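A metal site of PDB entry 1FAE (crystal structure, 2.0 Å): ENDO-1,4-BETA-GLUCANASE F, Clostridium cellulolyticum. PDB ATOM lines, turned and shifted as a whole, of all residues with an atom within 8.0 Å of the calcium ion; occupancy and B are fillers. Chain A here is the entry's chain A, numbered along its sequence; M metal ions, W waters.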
ATOM      1  N   GLN A 116      11.935  11.094   5.636  1.00  0.00           N
ATOM      2  CA  GLN A 116      10.791  11.943   5.961  1.00  0.00           C
ATOM      3  C   GLN A 116      10.866  12.697   7.302  1.00  0.00           C
ATOM      4  O   GLN A 116       9.907  13.334   7.713  1.00  0.00           O
ATOM      5  CB  GLN A 116       9.496  11.131   5.879  1.00  0.00           C
ATOM      6  CG  GLN A 116       9.017  10.850   4.436  1.00  0.00           C
ATOM      7  CD  GLN A 116       9.968   9.966   3.628  1.00  0.00           C
ATOM      8  OE1 GLN A 116      10.153   8.792   3.930  1.00  0.00           O
ATOM      9  NE2 GLN A 116      10.579  10.541   2.588  1.00  0.00           N
ATOM     10  N   ASP A 117      11.995  12.620   7.974  1.00  0.00           N
ATOM     11  CA  ASP A 117      12.174  13.319   9.232  1.00  0.00           C
ATOM     12  C   ASP A 117      13.644  13.652   9.305  1.00  0.00           C
ATOM     13  O   ASP A 117      14.500  12.795   9.036  1.00  0.00           O
ATOM     14  CB  ASP A 117      11.778  12.440  10.419  1.00  0.00           C
ATOM     15  CG  ASP A 117      11.648  13.249  11.699  1.00  0.00           C
ATOM     16  OD1 ASP A 117      10.524  13.679  12.024  1.00  0.00           O
ATOM     17  OD2 ASP A 117      12.673  13.503  12.356  1.00  0.00           O
ATOM     18  N   PRO A 118      13.970  14.908   9.628  1.00  0.00           N
ATOM     19  CA  PRO A 118      15.376  15.309   9.722  1.00  0.00           C
ATOM     20  C   PRO A 118      16.190  14.478  10.712  1.00  0.00           C
ATOM     21  O   PRO A 118      17.421  14.450  10.625  1.00  0.00           O
ATOM     22  CB  PRO A 118      15.286  16.769  10.164  1.00  0.00           C
ATOM     23  CG  PRO A 118      13.997  17.217   9.552  1.00  0.00           C
ATOM     24  CD  PRO A 118      13.082  16.058   9.850  1.00  0.00           C
ATOM     25  N   GLY A 183      15.436  16.676   3.739  1.00  0.00           N
ATOM     26  CA  GLY A 183      14.103  16.217   3.405  1.00  0.00           C
ATOM     27  C   GLY A 183      12.896  17.113   3.544  1.00  0.00           C
ATOM     28  O   GLY A 183      12.978  18.258   3.985  1.00  0.00           O
ATOM     29  N   GLU A 184      11.753  16.510   3.213  1.00  0.00           N
ATOM     30  CA  GLU A 184      10.463  17.179   3.226  1.00  0.00           C
ATOM     31  C   GLU A 184      10.011  17.826   4.532  1.00  0.00           C
ATOM     32  O   GLU A 184       9.270  18.806   4.519  1.00  0.00           O
ATOM     33  CB  GLU A 184       9.370  16.241   2.693  1.00  0.00           C
ATOM     34  CG  GLU A 184       9.014  15.080   3.585  1.00  0.00           C
ATOM     35  CD  GLU A 184       7.790  14.308   3.088  1.00  0.00           C
ATOM     36  OE1 GLU A 184       7.501  14.338   1.882  1.00  0.00           O
ATOM     37  OE2 GLU A 184       7.099  13.688   3.920  1.00  0.00           O
ATOM     38  N   GLN A 185      10.423  17.258   5.663  1.00  0.00           N
ATOM     39  CA  GLN A 185      10.030  17.832   6.936  1.00  0.00           C
ATOM     40  C   GLN A 185      10.995  18.878   7.464  1.00  0.00           C
ATOM     41  O   GLN A 185      10.815  19.403   8.554  1.00  0.00           O
ATOM     42  CB  GLN A 185       9.787  16.737   7.991  1.00  0.00           C
ATOM     43  CG  GLN A 185       8.333  16.329   8.074  1.00  0.00           C
ATOM     44  CD  GLN A 185       7.405  17.490   8.466  1.00  0.00           C
ATOM     45  OE1 GLN A 185       7.779  18.410   9.220  1.00  0.00           O
ATOM     46  NE2 GLN A 185       6.182  17.453   7.945  1.00  0.00           N
ATOM     47  N   GLU A 186      12.037  19.196   6.694  1.00  0.00           N
ATOM     48  CA  GLU A 186      12.965  20.218   7.157  1.00  0.00           C
ATOM     49  C   GLU A 186      12.541  21.588   6.655  1.00  0.00           C
ATOM     50  O   GLU A 186      12.834  21.964   5.528  1.00  0.00           O
ATOM     51  CB  GLU A 186      14.408  19.914   6.739  1.00  0.00           C
ATOM     52  CG  GLU A 186      15.407  20.863   7.382  1.00  0.00           C
ATOM     53  CD  GLU A 186      16.809  20.726   6.833  1.00  0.00           C
ATOM     54  OE1 GLU A 186      16.946  20.667   5.598  1.00  0.00           O
ATOM     55  OE2 GLU A 186      17.765  20.693   7.635  1.00  0.00           O
ATOM     56  N   SER A 187      11.803  22.321   7.493  1.00  0.00           N
ATOM     57  CA  SER A 187      11.349  23.661   7.128  1.00  0.00           C
ATOM     58  C   SER A 187      12.545  24.614   7.200  1.00  0.00           C
ATOM     59  O   SER A 187      13.647  24.230   7.596  1.00  0.00           O
ATOM     60  CB  SER A 187      10.264  24.139   8.091  1.00  0.00           C
ATOM     61  OG  SER A 187      10.789  24.397   9.384  1.00  0.00           O
ATOM     62  N   THR A 188      12.292  25.878   6.855  1.00  0.00           N
ATOM     63  CA  THR A 188      13.312  26.911   6.891  1.00  0.00           C
ATOM     64  C   THR A 188      13.791  27.079   8.334  1.00  0.00           C
ATOM     65  O   THR A 188      14.900  27.547   8.563  1.00  0.00           O
ATOM     66  CB  THR A 188      12.736  28.296   6.507  1.00  0.00           C
ATOM     67  OG1 THR A 188      11.782  28.152   5.459  1.00  0.00           O
ATOM     68  CG2 THR A 188      13.837  29.197   6.041  1.00  0.00           C
ATOM     69  N   TRP A 189      12.925  26.748   9.288  1.00  0.00           N
ATOM     70  CA  TRP A 189      13.227  26.869  10.712  1.00  0.00           C
ATOM     71  C   TRP A 189      14.079  25.730  11.273  1.00  0.00           C
ATOM     72  O   TRP A 189      14.624  25.849  12.369  1.00  0.00           O
ATOM     73  CB  TRP A 189      11.925  26.912  11.527  1.00  0.00           C
ATOM     74  CG  TRP A 189      10.996  27.994  11.095  1.00  0.00           C
ATOM     75  CD1 TRP A 189       9.940  27.878  10.229  1.00  0.00           C
ATOM     76  CD2 TRP A 189      11.048  29.373  11.486  1.00  0.00           C
ATOM     77  NE1 TRP A 189       9.350  29.108  10.043  1.00  0.00           N
ATOM     78  CE2 TRP A 189      10.011  30.043  10.797  1.00  0.00           C
ATOM     79  CE3 TRP A 189      11.887  30.114  12.337  1.00  0.00           C
ATOM     80  CZ2 TRP A 189       9.783  31.412  10.944  1.00  0.00           C
ATOM     81  CZ3 TRP A 189      11.663  31.478  12.476  1.00  0.00           C
ATOM     82  CH2 TRP A 189      10.611  32.106  11.791  1.00  0.00           C
ATOM     83  N   GLU A 190      14.225  24.653  10.508  1.00  0.00           N
ATOM     84  CA  GLU A 190      14.944  23.484  10.975  1.00  0.00           C
ATOM     85  C   GLU A 190      16.275  23.134  10.348  1.00  0.00           C
ATOM     86  O   GLU A 190      16.811  22.043  10.583  1.00  0.00           O
ATOM     87  CB  GLU A 190      14.004  22.298  10.862  1.00  0.00           C
ATOM     88  CG  GLU A 190      12.847  22.374  11.798  1.00  0.00           C
ATOM     89  CD  GLU A 190      11.726  21.508  11.336  1.00  0.00           C
ATOM     90  OE1 GLU A 190      11.619  20.364  11.808  1.00  0.00           O
ATOM     91  OE2 GLU A 190      10.948  21.979  10.479  1.00  0.00           O
ATOM     92  N   ALA A 404       6.883  19.542   2.930  1.00  0.00           N
ATOM     93  CA  ALA A 404       5.622  19.308   3.630  1.00  0.00           C
ATOM     94  C   ALA A 404       5.440  20.226   4.840  1.00  0.00           C
ATOM     95  O   ALA A 404       4.402  20.190   5.499  1.00  0.00           O
ATOM     96  CB  ALA A 404       5.532  17.847   4.082  1.00  0.00           C
ATOM     97  N   ASP A 405       6.434  21.081   5.117  1.00  0.00           N
ATOM     98  CA  ASP A 405       6.385  21.988   6.259  1.00  0.00           C
ATOM     99  C   ASP A 405       6.807  23.433   5.917  1.00  0.00           C
ATOM    100  O   ASP A 405       7.926  23.858   6.234  1.00  0.00           O
ATOM    101  CB  ASP A 405       7.287  21.406   7.352  1.00  0.00           C
ATOM    102  CG  ASP A 405       7.220  22.173   8.658  1.00  0.00           C
ATOM    103  OD1 ASP A 405       6.385  23.075   8.839  1.00  0.00           O
ATOM    104  OD2 ASP A 405       8.027  21.849   9.534  1.00  0.00           O
ATOM    105  N   PRO A 406       5.908  24.218   5.290  1.00  0.00           N
ATOM    106  CA  PRO A 406       4.550  23.819   4.901  1.00  0.00           C
ATOM    107  C   PRO A 406       4.527  23.172   3.503  1.00  0.00           C
ATOM    108  O   PRO A 406       5.548  23.153   2.804  1.00  0.00           O
ATOM    109  CB  PRO A 406       3.811  25.156   4.895  1.00  0.00           C
ATOM    110  CG  PRO A 406       4.842  26.084   4.334  1.00  0.00           C
ATOM    111  CD  PRO A 406       6.129  25.659   5.030  1.00  0.00           C
ATOM    112  N   ARG A 549       8.324  30.134  15.968  1.00  0.00           N
ATOM    113  CA  ARG A 549       9.361  29.122  15.765  1.00  0.00           C
ATOM    114  C   ARG A 549      10.792  29.664  15.954  1.00  0.00           C
ATOM    115  O   ARG A 549      11.750  28.898  16.085  1.00  0.00           O
ATOM    116  CB  ARG A 549       9.161  28.427  14.410  1.00  0.00           C
ATOM    117  CG  ARG A 549       7.746  27.831  14.270  1.00  0.00           C
ATOM    118  CD  ARG A 549       7.495  27.201  12.931  1.00  0.00           C
ATOM    119  NE  ARG A 549       8.219  25.940  12.780  1.00  0.00           N
ATOM    120  CZ  ARG A 549       7.970  25.036  11.842  1.00  0.00           C
ATOM    121  NH1 ARG A 549       7.024  25.243  10.940  1.00  0.00           N
ATOM    122  NH2 ARG A 549       8.646  23.892  11.827  1.00  0.00           N
ATOM    123  N   GLN A 553      11.296  26.392  18.071  1.00  0.00           N
ATOM    124  CA  GLN A 553      11.643  25.332  17.120  1.00  0.00           C
ATOM    125  C   GLN A 553      12.986  24.698  17.403  1.00  0.00           C
ATOM    126  O   GLN A 553      14.027  25.353  17.283  1.00  0.00           O
ATOM    127  CB  GLN A 553      11.654  25.840  15.674  1.00  0.00           C
ATOM    128  CG  GLN A 553      11.999  24.752  14.651  1.00  0.00           C
ATOM    129  CD  GLN A 553      10.954  23.655  14.602  1.00  0.00           C
ATOM    130  OE1 GLN A 553       9.803  23.910  14.264  1.00  0.00           O
ATOM    131  NE2 GLN A 553      11.350  22.435  14.939  1.00  0.00           N
ATOM    132  N   GLU A 554      12.967  23.437  17.782  1.00  0.00           N
ATOM    133  CA  GLU A 554      14.199  22.728  18.055  1.00  0.00           C
ATOM    134  C   GLU A 554      14.830  22.281  16.737  1.00  0.00           C
ATOM    135  O   GLU A 554      14.129  21.924  15.794  1.00  0.00           O
ATOM    136  CB  GLU A 554      13.931  21.519  18.939  1.00  0.00           C
ATOM    137  CG  GLU A 554      15.194  20.806  19.375  1.00  0.00           C
ATOM    138  CD  GLU A 554      14.908  19.647  20.310  1.00  0.00           C
ATOM    139  OE1 GLU A 554      14.144  19.850  21.283  1.00  0.00           O
ATOM    140  OE2 GLU A 554      15.469  18.551  20.071  1.00  0.00           O
HETATM  141 CA    CA M   1       9.351  19.940  10.423  1.00  0.00          CA
HETATM  142  O   HOH W   1       9.887  17.751  11.385  1.00  0.00           O
HETATM  143  O   HOH W   2       8.283  20.542  12.509  1.00  0.00           O
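The calcium ion is bound by water W2 (2.4 Å), the backbone carbonyl oxygen (O) of Gln 185 (2.4 Å), water W1 (2.5 Å), the side-chain carboxylate (OD2) of Asp 405 (2.5 Å), the side-chain amide oxygen (OE1) of Gln 185 (2.5 Å), the side-chain carboxylate (OE2) of Glu 190 (2.6 Å) and the side-chain carboxylate (OE1) of Glu 190 (2.7 Å).
The calcium ion has seven donor atoms within binding distance.
The side-chain carboxylate (OD1) of Asp 405 lies within salt-bridge range of the guanidinium group (NH1) of Arg 549 (3.1 Å).
The guanidinium group of Arg 549 sits close to the side-chain carboxylate of Glu 190.
The side-chain hydroxyl (OG) of Ser 187 sits close to the side-chain carboxylate (OE2) of Glu 190 (2.7 Å).
The nearest printed residue that does not touch the calcium ion is Arg 549 (4.3 Å).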
